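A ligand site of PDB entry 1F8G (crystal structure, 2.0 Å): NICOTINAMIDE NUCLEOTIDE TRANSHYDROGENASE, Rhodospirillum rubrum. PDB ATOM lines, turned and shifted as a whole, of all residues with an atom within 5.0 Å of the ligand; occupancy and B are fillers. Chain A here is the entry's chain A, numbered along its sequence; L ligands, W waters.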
ATOM      1  N   ARG A 127     -15.236 -24.064 -22.161  1.00  0.00           N
ATOM      2  CA  ARG A 127     -15.567 -22.675 -21.852  1.00  0.00           C
ATOM      3  C   ARG A 127     -16.439 -22.063 -22.924  1.00  0.00           C
ATOM      4  O   ARG A 127     -16.029 -21.243 -23.751  1.00  0.00           O
ATOM      5  CB  ARG A 127     -14.305 -21.867 -21.583  1.00  0.00           C
ATOM      6  CG  ARG A 127     -13.613 -22.221 -20.273  1.00  0.00           C
ATOM      7  CD  ARG A 127     -12.371 -23.050 -20.511  1.00  0.00           C
ATOM      8  N   GLN A 132     -21.716 -22.364 -18.759  1.00  0.00           N
ATOM      9  CA  GLN A 132     -21.393 -21.621 -17.539  1.00  0.00           C
ATOM     10  C   GLN A 132     -22.085 -22.154 -16.296  1.00  0.00           C
ATOM     11  O   GLN A 132     -21.498 -22.157 -15.199  1.00  0.00           O
ATOM     12  CB  GLN A 132     -21.750 -20.128 -17.698  1.00  0.00           C
ATOM     13  CG  GLN A 132     -20.743 -19.381 -18.578  1.00  0.00           C
ATOM     14  CD  GLN A 132     -21.187 -17.960 -18.896  1.00  0.00           C
ATOM     15  OE1 GLN A 132     -22.310 -17.709 -19.351  1.00  0.00           O
ATOM     16  NE2 GLN A 132     -20.268 -17.026 -18.674  1.00  0.00           N
ATOM     17  N   ASP A 135     -20.160 -25.136 -14.896  1.00  0.00           N
ATOM     18  CA  ASP A 135     -18.739 -24.990 -14.611  1.00  0.00           C
ATOM     19  C   ASP A 135     -18.354 -24.957 -13.151  1.00  0.00           C
ATOM     20  O   ASP A 135     -18.556 -23.934 -12.478  1.00  0.00           O
ATOM     21  CB  ASP A 135     -18.246 -23.742 -15.379  1.00  0.00           C
ATOM     22  CG  ASP A 135     -16.731 -23.696 -15.421  1.00  0.00           C
ATOM     23  OD1 ASP A 135     -16.060 -23.266 -14.469  1.00  0.00           O
ATOM     24  OD2 ASP A 135     -16.127 -24.127 -16.427  1.00  0.00           O
ATOM     25  N   LEU A 137     -15.250 -24.941 -11.943  1.00  0.00           N
ATOM     26  CA  LEU A 137     -14.142 -24.024 -11.632  1.00  0.00           C
ATOM     27  C   LEU A 137     -14.660 -22.635 -11.263  1.00  0.00           C
ATOM     28  O   LEU A 137     -14.139 -22.059 -10.312  1.00  0.00           O
ATOM     29  CB  LEU A 137     -13.122 -23.989 -12.773  1.00  0.00           C
ATOM     30  CG  LEU A 137     -12.462 -25.339 -13.062  1.00  0.00           C
ATOM     31  CD1 LEU A 137     -11.541 -25.280 -14.280  1.00  0.00           C
ATOM     32  CD2 LEU A 137     -11.694 -25.854 -11.847  1.00  0.00           C
ATOM     33  N   SER A 138     -15.622 -22.068 -11.988  1.00  0.00           N
ATOM     34  CA  SER A 138     -16.069 -20.711 -11.645  1.00  0.00           C
ATOM     35  C   SER A 138     -16.965 -20.659 -10.424  1.00  0.00           C
ATOM     36  O   SER A 138     -16.841 -19.688  -9.648  1.00  0.00           O
ATOM     37  CB  SER A 138     -16.713 -20.000 -12.839  1.00  0.00           C
ATOM     38  OG  SER A 138     -17.826 -20.722 -13.293  1.00  0.00           O
ATOM     39  N   SER A 141     -14.386 -20.950  -7.608  1.00  0.00           N
ATOM     40  CA  SER A 141     -13.517 -19.807  -7.619  1.00  0.00           C
ATOM     41  C   SER A 141     -14.146 -18.524  -7.078  1.00  0.00           C
ATOM     42  O   SER A 141     -13.501 -17.696  -6.441  1.00  0.00           O
ATOM     43  CB  SER A 141     -13.221 -19.349  -9.095  1.00  0.00           C
ATOM     44  OG  SER A 141     -12.292 -20.271  -9.568  1.00  0.00           O
ATOM     45  N   PHE A 178      -4.519  -9.078  -7.586  1.00  0.00           N
ATOM     46  CA  PHE A 178      -3.698  -9.489  -8.709  1.00  0.00           C
ATOM     47  C   PHE A 178      -4.365 -10.667  -9.419  1.00  0.00           C
ATOM     48  O   PHE A 178      -4.437 -11.749  -8.849  1.00  0.00           O
ATOM     49  CB  PHE A 178      -2.329  -9.968  -8.249  1.00  0.00           C
ATOM     50  CG  PHE A 178      -1.326  -9.004  -7.735  1.00  0.00           C
ATOM     51  CD1 PHE A 178      -1.453  -8.468  -6.448  1.00  0.00           C
ATOM     52  CD2 PHE A 178      -0.226  -8.646  -8.491  1.00  0.00           C
ATOM     53  CE1 PHE A 178      -0.513  -7.589  -5.952  1.00  0.00           C
ATOM     54  CE2 PHE A 178       0.727  -7.768  -8.005  1.00  0.00           C
ATOM     55  CZ  PHE A 178       0.562  -7.240  -6.741  1.00  0.00           C
ATOM     56  N   GLY A 179      -4.803 -10.456 -10.645  1.00  0.00           N
ATOM     57  CA  GLY A 179      -5.482 -11.486 -11.416  1.00  0.00           C
ATOM     58  C   GLY A 179      -6.982 -11.220 -11.247  1.00  0.00           C
ATOM     59  O   GLY A 179      -7.516 -11.308 -10.145  1.00  0.00           O
ATOM     60  N   VAL A 180      -7.612 -10.787 -12.335  1.00  0.00           N
ATOM     61  CA  VAL A 180      -9.040 -10.448 -12.242  1.00  0.00           C
ATOM     62  C   VAL A 180      -9.877 -11.427 -13.045  1.00  0.00           C
ATOM     63  O   VAL A 180     -10.569 -11.072 -14.007  1.00  0.00           O
ATOM     64  CB  VAL A 180      -9.287  -8.998 -12.666  1.00  0.00           C
ATOM     65  CG1 VAL A 180     -10.701  -8.501 -12.356  1.00  0.00           C
ATOM     66  CG2 VAL A 180      -8.287  -8.043 -12.000  1.00  0.00           C
ATOM     67  N   GLY A 181      -9.768 -12.704 -12.658  1.00  0.00           N
ATOM     68  CA  GLY A 181     -10.565 -13.772 -13.254  1.00  0.00           C
ATOM     69  C   GLY A 181     -11.825 -13.861 -12.371  1.00  0.00           C
ATOM     70  O   GLY A 181     -12.201 -12.901 -11.703  1.00  0.00           O
ATOM     71  N   VAL A 182     -12.417 -15.048 -12.276  1.00  0.00           N
ATOM     72  CA  VAL A 182     -13.615 -15.207 -11.448  1.00  0.00           C
ATOM     73  C   VAL A 182     -13.325 -14.884  -9.989  1.00  0.00           C
ATOM     74  O   VAL A 182     -14.098 -14.134  -9.367  1.00  0.00           O
ATOM     75  CB  VAL A 182     -14.177 -16.628 -11.647  1.00  0.00           C
ATOM     76  CG1 VAL A 182     -15.397 -16.895 -10.770  1.00  0.00           C
ATOM     77  CG2 VAL A 182     -14.547 -16.813 -13.139  1.00  0.00           C
ATOM     78  N   ALA A 183     -12.272 -15.438  -9.394  1.00  0.00           N
ATOM     79  CA  ALA A 183     -11.937 -15.193  -8.002  1.00  0.00           C
ATOM     80  C   ALA A 183     -11.573 -13.731  -7.745  1.00  0.00           C
ATOM     81  O   ALA A 183     -12.106 -13.131  -6.815  1.00  0.00           O
ATOM     82  CB  ALA A 183     -10.794 -16.073  -7.536  1.00  0.00           C
ATOM     83  N   THR A 201      -5.000  -5.563 -10.980  1.00  0.00           N
ATOM     84  CA  THR A 201      -4.188  -5.673 -12.184  1.00  0.00           C
ATOM     85  C   THR A 201      -4.320  -7.072 -12.784  1.00  0.00           C
ATOM     86  O   THR A 201      -4.473  -8.056 -12.061  1.00  0.00           O
ATOM     87  CB  THR A 201      -2.700  -5.383 -11.920  1.00  0.00           C
ATOM     88  OG1 THR A 201      -2.002  -5.376 -13.171  1.00  0.00           O
ATOM     89  CG2 THR A 201      -2.014  -6.433 -11.062  1.00  0.00           C
ATOM     90  N   ASP A 202      -4.260  -7.148 -14.107  1.00  0.00           N
ATOM     91  CA  ASP A 202      -4.334  -8.396 -14.849  1.00  0.00           C
ATOM     92  C   ASP A 202      -3.637  -8.176 -16.199  1.00  0.00           C
ATOM     93  O   ASP A 202      -3.617  -7.050 -16.678  1.00  0.00           O
ATOM     94  CB  ASP A 202      -5.781  -8.789 -15.134  1.00  0.00           C
ATOM     95  CG  ASP A 202      -5.967 -10.240 -15.531  1.00  0.00           C
ATOM     96  OD1 ASP A 202      -6.706 -10.959 -14.828  1.00  0.00           O
ATOM     97  OD2 ASP A 202      -5.395 -10.713 -16.546  1.00  0.00           O
ATOM     98  N   VAL A 203      -3.200  -9.262 -16.832  1.00  0.00           N
ATOM     99  CA  VAL A 203      -2.589  -9.177 -18.149  1.00  0.00           C
ATOM    100  C   VAL A 203      -3.653  -9.035 -19.239  1.00  0.00           C
ATOM    101  O   VAL A 203      -3.298  -8.639 -20.350  1.00  0.00           O
ATOM    102  CB  VAL A 203      -1.703 -10.389 -18.459  1.00  0.00           C
ATOM    103  CG1 VAL A 203      -0.580 -10.478 -17.438  1.00  0.00           C
ATOM    104  CG2 VAL A 203      -2.474 -11.699 -18.503  1.00  0.00           C
ATOM    105  N   ARG A 204      -4.922  -9.319 -18.969  1.00  0.00           N
ATOM    106  CA  ARG A 204      -5.957  -9.219 -19.997  1.00  0.00           C
ATOM    107  C   ARG A 204      -6.568  -7.831 -19.976  1.00  0.00           C
ATOM    108  O   ARG A 204      -7.099  -7.367 -18.962  1.00  0.00           O
ATOM    109  CB  ARG A 204      -7.005 -10.322 -19.805  1.00  0.00           C
ATOM    110  CG  ARG A 204      -6.457 -11.729 -20.055  1.00  0.00           C
ATOM    111  CD  ARG A 204      -7.541 -12.798 -20.020  1.00  0.00           C
ATOM    112  NE  ARG A 204      -8.180 -12.877 -18.702  1.00  0.00           N
ATOM    113  CZ  ARG A 204      -9.395 -12.431 -18.402  1.00  0.00           C
ATOM    114  NH1 ARG A 204     -10.171 -11.869 -19.341  1.00  0.00           N
ATOM    115  NH2 ARG A 204      -9.851 -12.557 -17.164  1.00  0.00           N
ATOM    116  N   THR A 207     -10.314  -6.777 -18.705  1.00  0.00           N
ATOM    117  CA  THR A 207     -10.507  -6.800 -17.260  1.00  0.00           C
ATOM    118  C   THR A 207     -10.706  -5.419 -16.676  1.00  0.00           C
ATOM    119  O   THR A 207     -11.470  -5.211 -15.738  1.00  0.00           O
ATOM    120  CB  THR A 207      -9.258  -7.540 -16.733  1.00  0.00           C
ATOM    121  OG1 THR A 207      -9.557  -8.952 -16.734  1.00  0.00           O
ATOM    122  CG2 THR A 207      -8.805  -7.114 -15.384  1.00  0.00           C
ATOM    123  N   GLY A 233      -9.919 -19.464 -25.088  1.00  0.00           N
ATOM    124  CA  GLY A 233     -10.805 -19.891 -24.029  1.00  0.00           C
ATOM    125  C   GLY A 233     -11.104 -18.853 -22.965  1.00  0.00           C
ATOM    126  O   GLY A 233     -11.682 -19.165 -21.910  1.00  0.00           O
ATOM    127  N   GLY A 234     -10.690 -17.606 -23.151  1.00  0.00           N
ATOM    128  CA  GLY A 234     -10.889 -16.514 -22.208  1.00  0.00           C
ATOM    129  C   GLY A 234      -9.780 -16.509 -21.159  1.00  0.00           C
ATOM    130  O   GLY A 234      -9.823 -15.884 -20.108  1.00  0.00           O
ATOM    131  N   TYR A 235      -8.718 -17.214 -21.504  1.00  0.00           N
ATOM    132  CA  TYR A 235      -7.568 -17.472 -20.693  1.00  0.00           C
ATOM    133  C   TYR A 235      -6.300 -16.676 -20.937  1.00  0.00           C
ATOM    134  O   TYR A 235      -5.961 -16.378 -22.088  1.00  0.00           O
ATOM    135  CB  TYR A 235      -7.185 -18.941 -20.926  1.00  0.00           C
ATOM    136  CG  TYR A 235      -8.010 -19.956 -20.163  1.00  0.00           C
ATOM    137  CD1 TYR A 235      -8.807 -20.881 -20.811  1.00  0.00           C
ATOM    138  CD2 TYR A 235      -7.965 -19.970 -18.776  1.00  0.00           C
ATOM    139  CE1 TYR A 235      -9.532 -21.801 -20.079  1.00  0.00           C
ATOM    140  CE2 TYR A 235      -8.696 -20.883 -18.042  1.00  0.00           C
ATOM    141  CZ  TYR A 235      -9.484 -21.798 -18.709  1.00  0.00           C
ATOM    142  OH  TYR A 235     -10.217 -22.722 -17.987  1.00  0.00           O
ATOM    143  N   ALA A 236      -5.554 -16.453 -19.854  1.00  0.00           N
ATOM    144  CA  ALA A 236      -4.309 -15.717 -19.999  1.00  0.00           C
ATOM    145  C   ALA A 236      -3.069 -16.597 -19.992  1.00  0.00           C
ATOM    146  O   ALA A 236      -3.102 -17.828 -19.984  1.00  0.00           O
ATOM    147  CB  ALA A 236      -4.162 -14.660 -18.918  1.00  0.00           C
ATOM    148  N   LYS A 237      -1.949 -15.857 -20.014  1.00  0.00           N
ATOM    149  CA  LYS A 237      -0.681 -16.527 -20.116  1.00  0.00           C
ATOM    150  C   LYS A 237       0.593 -15.918 -19.551  1.00  0.00           C
ATOM    151  O   LYS A 237       0.840 -15.007 -18.797  1.00  0.00           O
ATOM    152  CB  LYS A 237      -0.452 -16.717 -21.646  1.00  0.00           C
ATOM    153  CG  LYS A 237      -0.609 -18.171 -22.063  1.00  0.00           C
ATOM    154  CD  LYS A 237      -0.286 -18.372 -23.534  1.00  0.00           C
ATOM    155  CE  LYS A 237      -0.502 -19.837 -23.903  1.00  0.00           C
ATOM    156  NZ  LYS A 237      -0.028 -20.130 -25.280  1.00  0.00           N
ATOM    157  N   GLN A 247       5.558  -5.013 -15.174  1.00  0.00           N
ATOM    158  CA  GLN A 247       4.361  -5.138 -14.328  1.00  0.00           C
ATOM    159  C   GLN A 247       4.721  -4.890 -12.874  1.00  0.00           C
ATOM    160  O   GLN A 247       3.958  -4.281 -12.118  1.00  0.00           O
ATOM    161  CB  GLN A 247       3.717  -6.505 -14.516  1.00  0.00           C
ATOM    162  CG  GLN A 247       2.567  -6.859 -13.586  1.00  0.00           C
ATOM    163  CD  GLN A 247       2.151  -8.312 -13.760  1.00  0.00           C
ATOM    164  OE1 GLN A 247       1.047  -8.629 -14.211  1.00  0.00           O
ATOM    165  NE2 GLN A 247       3.035  -9.227 -13.405  1.00  0.00           N
ATOM    166  N   THR A 264      -4.435 -14.166  -7.363  1.00  0.00           N
ATOM    167  CA  THR A 264      -5.246 -15.252  -7.861  1.00  0.00           C
ATOM    168  C   THR A 264      -4.828 -15.761  -9.242  1.00  0.00           C
ATOM    169  O   THR A 264      -5.587 -16.528  -9.837  1.00  0.00           O
ATOM    170  CB  THR A 264      -6.710 -14.759  -8.043  1.00  0.00           C
ATOM    171  OG1 THR A 264      -6.753 -13.981  -9.259  1.00  0.00           O
ATOM    172  CG2 THR A 264      -7.267 -13.910  -6.928  1.00  0.00           C
ATOM    173  N   ALA A 265      -3.701 -15.323  -9.777  1.00  0.00           N
ATOM    174  CA  ALA A 265      -3.336 -15.652 -11.142  1.00  0.00           C
ATOM    175  C   ALA A 265      -2.864 -17.073 -11.385  1.00  0.00           C
ATOM    176  O   ALA A 265      -2.035 -17.644 -10.703  1.00  0.00           O
ATOM    177  CB  ALA A 265      -2.282 -14.663 -11.643  1.00  0.00           C
ATOM    178  N   LEU A 266      -3.402 -17.676 -12.434  1.00  0.00           N
ATOM    179  CA  LEU A 266      -3.075 -19.026 -12.889  1.00  0.00           C
ATOM    180  C   LEU A 266      -2.840 -18.998 -14.404  1.00  0.00           C
ATOM    181  O   LEU A 266      -3.282 -18.057 -15.078  1.00  0.00           O
ATOM    182  CB  LEU A 266      -4.247 -19.948 -12.609  1.00  0.00           C
ATOM    183  CG  LEU A 266      -4.332 -20.877 -11.414  1.00  0.00           C
ATOM    184  CD1 LEU A 266      -3.586 -20.418 -10.190  1.00  0.00           C
ATOM    185  CD2 LEU A 266      -5.796 -21.161 -11.104  1.00  0.00           C
ATOM    186  N   ILE A 267      -2.137 -19.983 -14.922  1.00  0.00           N
ATOM    187  CA  ILE A 267      -1.863 -20.156 -16.336  1.00  0.00           C
ATOM    188  C   ILE A 267      -2.091 -21.648 -16.670  1.00  0.00           C
ATOM    189  O   ILE A 267      -1.430 -22.500 -16.089  1.00  0.00           O
ATOM    190  CB  ILE A 267      -0.403 -19.843 -16.742  1.00  0.00           C
ATOM    191  CG1 ILE A 267      -0.043 -18.385 -16.536  1.00  0.00           C
ATOM    192  CG2 ILE A 267      -0.176 -20.216 -18.208  1.00  0.00           C
ATOM    193  CD1 ILE A 267       1.441 -18.086 -16.445  1.00  0.00           C
ATOM    194  N   PRO A 273       2.226 -17.792 -12.056  1.00  0.00           N
ATOM    195  CA  PRO A 273       3.196 -16.744 -12.291  1.00  0.00           C
ATOM    196  C   PRO A 273       3.581 -16.064 -10.981  1.00  0.00           C
ATOM    197  O   PRO A 273       2.746 -15.907 -10.075  1.00  0.00           O
ATOM    198  CB  PRO A 273       2.477 -15.793 -13.240  1.00  0.00           C
ATOM    199  CG  PRO A 273       1.024 -15.993 -12.954  1.00  0.00           C
ATOM    200  CD  PRO A 273       0.887 -17.461 -12.588  1.00  0.00           C
ATOM    201  N   LEU A 275       4.171 -13.016  -8.970  1.00  0.00           N
ATOM    202  CA  LEU A 275       3.692 -11.632  -9.041  1.00  0.00           C
ATOM    203  C   LEU A 275       4.187 -10.790  -7.881  1.00  0.00           C
ATOM    204  O   LEU A 275       4.248  -9.551  -7.958  1.00  0.00           O
ATOM    205  CB  LEU A 275       2.166 -11.634  -9.122  1.00  0.00           C
ATOM    206  CG  LEU A 275       1.552 -12.391 -10.306  1.00  0.00           C
ATOM    207  CD1 LEU A 275       0.034 -12.306 -10.318  1.00  0.00           C
ATOM    208  CD2 LEU A 275       2.071 -11.865 -11.644  1.00  0.00           C
HETATM  209  P1  LIG L   1      -7.795 -18.124 -14.118  1.00  0.00           P
HETATM  210  O1  LIG L   1      -8.166 -18.816 -12.855  1.00  0.00           O
HETATM  211  O2  LIG L   1      -7.150 -19.106 -15.014  1.00  0.00           O
HETATM  212  O3  LIG L   1      -6.748 -16.941 -13.884  1.00  0.00           O
HETATM  213  C1  LIG L   1      -7.049 -15.855 -12.944  1.00  0.00           C
HETATM  214  C2  LIG L   1      -6.739 -14.551 -13.670  1.00  0.00           C
HETATM  215  O4  LIG L   1      -5.266 -14.458 -13.611  1.00  0.00           O
HETATM  216  C3  LIG L   1      -7.091 -14.496 -15.162  1.00  0.00           C
HETATM  217  O5  LIG L   1      -7.968 -13.424 -15.495  1.00  0.00           O
HETATM  218  C4  LIG L   1      -5.759 -14.275 -15.874  1.00  0.00           C
HETATM  219  O6  LIG L   1      -5.802 -13.388 -16.976  1.00  0.00           O
HETATM  220  C5  LIG L   1      -4.889 -13.726 -14.753  1.00  0.00           C
HETATM  221  N1  LIG L   1      -3.437 -13.810 -14.956  1.00  0.00           N
HETATM  222  C6  LIG L   1      -2.689 -14.780 -15.532  1.00  0.00           C
HETATM  223  N2  LIG L   1      -1.387 -14.493 -15.536  1.00  0.00           N
HETATM  224  C7  LIG L   1      -1.315 -13.265 -14.941  1.00  0.00           C
HETATM  225  C8  LIG L   1      -0.207 -12.439 -14.659  1.00  0.00           C
HETATM  226  N3  LIG L   1       1.027 -12.796 -14.982  1.00  0.00           N
HETATM  227  N4  LIG L   1      -0.450 -11.258 -14.056  1.00  0.00           N
HETATM  228  C9  LIG L   1      -1.760 -10.948 -13.743  1.00  0.00           C
HETATM  229  N5  LIG L   1      -2.843 -11.639 -13.956  1.00  0.00           N
HETATM  230  C10 LIG L   1      -2.555 -12.812 -14.578  1.00  0.00           C
HETATM  231  O7  LIG L   1      -9.040 -17.320 -14.713  1.00  0.00           O
HETATM  232  P2  LIG L   1     -10.616 -17.537 -14.666  1.00  0.00           P
HETATM  233  O8  LIG L   1     -11.159 -17.357 -13.314  1.00  0.00           O
HETATM  234  O9  LIG L   1     -10.891 -18.932 -15.093  1.00  0.00           O
HETATM  235  O10 LIG L   1     -11.122 -16.406 -15.648  1.00  0.00           O
HETATM  236  C11 LIG L   1     -10.654 -16.272 -17.007  1.00  0.00           C
HETATM  237  C12 LIG L   1     -11.787 -15.763 -17.868  1.00  0.00           C
HETATM  238  O11 LIG L   1     -12.497 -16.910 -18.398  1.00  0.00           O
HETATM  239  C13 LIG L   1     -12.851 -14.904 -17.163  1.00  0.00           C
HETATM  240  O12 LIG L   1     -13.447 -14.049 -18.142  1.00  0.00           O
HETATM  241  C14 LIG L   1     -13.874 -15.995 -16.774  1.00  0.00           C
HETATM  242  O13 LIG L   1     -15.144 -15.390 -16.533  1.00  0.00           O
HETATM  243  C15 LIG L   1     -13.881 -16.763 -18.110  1.00  0.00           C
HETATM  244  N6  LIG L   1     -14.404 -18.134 -17.961  1.00  0.00           N
HETATM  245  C16 LIG L   1     -13.770 -18.936 -17.063  1.00  0.00           C
HETATM  246  C17 LIG L   1     -14.226 -20.209 -16.883  1.00  0.00           C
HETATM  247  C18 LIG L   1     -13.610 -21.268 -15.905  1.00  0.00           C
HETATM  248  O14 LIG L   1     -13.508 -22.446 -16.264  1.00  0.00           O
HETATM  249  N7  LIG L   1     -13.210 -20.795 -14.721  1.00  0.00           N
HETATM  250  C19 LIG L   1     -15.324 -20.749 -17.585  1.00  0.00           C
HETATM  251  C20 LIG L   1     -15.896 -19.836 -18.480  1.00  0.00           C
HETATM  252  C21 LIG L   1     -15.526 -18.545 -18.718  1.00  0.00           C
HETATM  253  O   HOH W   1     -12.440 -19.750 -12.331  1.00  0.00           O
HETATM  254  O   HOH W   2      -9.659 -21.390 -12.719  1.00  0.00           O
HETATM  255  O   HOH W   3      -5.284 -17.865 -17.246  1.00  0.00           O
HETATM  256  O   HOH W   4     -13.748 -25.555 -17.171  1.00  0.00           O
HETATM  257  O   HOH W   5     -14.088 -14.926 -21.119  1.00  0.00           O
HETATM  258  O   HOH W   6     -12.784 -10.715 -18.942  1.00  0.00           O
HETATM  259  O   HOH W   7     -10.170 -16.986 -10.778  1.00  0.00           O
HETATM  260  O   HOH W   8      -7.813 -18.251 -10.089  1.00  0.00           O
HETATM  261  O   HOH W   9      -9.051 -14.397 -10.576  1.00  0.00           O
HETATM  262  O   HOH W  10     -18.288 -21.677 -19.503  1.00  0.00           O
HETATM  263  O   HOH W  11       3.548 -11.380 -15.068  1.00  0.00           O
HETATM  264  O   HOH W  12      -6.149 -21.583 -15.568  1.00  0.00           O
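NH2 of Arg 204 sits at hydrogen-bond distance from O5 of the ligand, 2.7 Å away.
The side-chain carboxylate of Asp 202 lies within hydrogen-bond range of an oxygen (O6) of the ligand, at 2.7 Å.
N of Val 182 lies within hydrogen-bond range of O8 of the ligand (2.8 Å).
N4 of the ligand lies close to OE1 of Gln 247 (3.0 Å).
The backbone NH (N) of Gly 181 sits at hydrogen-bond distance from an oxygen (O5) of the ligand (3.4 Å).
The backbone NH (N) of Arg 204 is in hydrogen-bond range of the side-chain carboxylate (OD2) of Asp 202 (2.8 Å).
OD1 of Asp 202 lies within hydrogen-bond range of N of Val 180 (2.7 Å).
The side-chain carboxylate of Asp 135 lies within hydrogen-bond range of the backbone NH of Leu 137.
The backbone NH of Ser 138 lies within hydrogen-bond range of the side-chain carboxylate of Asp 135 (2.8 Å).
The side-chain hydroxyl of Thr 264 is in hydrogen-bond range of the backbone carbonyl oxygen of Gly 179, 2.9 Å away.
The backbone carbonyl oxygen of Phe 178 is in hydrogen-bond range of the backbone NH of Thr 264 (2.8 Å).
The backbone NH (N) of Gly 179 lies within hydrogen-bond range of the backbone carbonyl oxygen (O) of Thr 201.
The backbone carbonyl oxygen of Leu 137 lies within hydrogen-bond range of the side-chain hydroxyl of Ser 141, at 2.7 Å.
OD2 of Asp 135 lies close to O14 of the ligand (3.1 Å).
O of Gly 234 sits close to O11 of the ligand, 3.3 Å away.
Merely in contact with the ligand: Ala 236 (2.8 Å), Ala 265 (3.4 Å), Leu 266 (3.4 Å), Val 203 (3.4 Å), Thr 264 (3.5 Å), Arg 127 (3.5 Å), Leu 275 (3.5 Å), Gly 179 (3.7 Å), Val 180 (3.7 Å), Tyr 235 (3.7 Å), Leu 137 (3.7 Å), Pro 273 (3.8 Å), Ser 138 (3.9 Å) and Lys 237 (3.98 Å).
Hydrophobic or aromatic side chains that line the ligand: Leu 137, Val 182, Val 203, Tyr 235, Ala 236, Ala 265, Leu 266, Pro 273 and Leu 275.
21 residues have an atom within 4 Å of the ligand: Arg 127, Asp 135, Leu 137, Ser 138, Gly 179, Val 180, Gly 181, Val 182, Asp 202, Val 203, Arg 204, Gly 234, Tyr 235, Ala 236, Lys 237, Gln 247, Thr 264, Ala 265, Leu 266, Pro 273 and Leu 275.
The nearest printed residue that does not touch the ligand is Ile 267 (4.2 Å).
Water W7 lies within hydrogen-bond range of an oxygen (O8) of the ligand (2.7 Å), the backbone NH (N) of Ala 183 (3.0 Å) and the backbone NH (N) of Val 182 (3.3 Å).
Water W8 lies within hydrogen-bond range of O of Thr 264 (2.8 Å) and O1 of the ligand (2.8 Å).
Water W11 bridges the side-chain amide nitrogen of Gln 247 (2.8 Å) and a nitrogen (N3) of the ligand (2.9 Å).
Water W3 lies within hydrogen-bond range of O of Leu 266 (3.0 Å), N of Ala 236 (3.0 Å) and O2 of the ligand (3.2 Å).
Water W4 lies within hydrogen-bond range of OD2 of Asp 135 (2.9 Å) and O14 of the ligand (3.2 Å).
Water W6 lies within hydrogen-bond range of NH1 of Arg 204 and O12 of the ligand.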
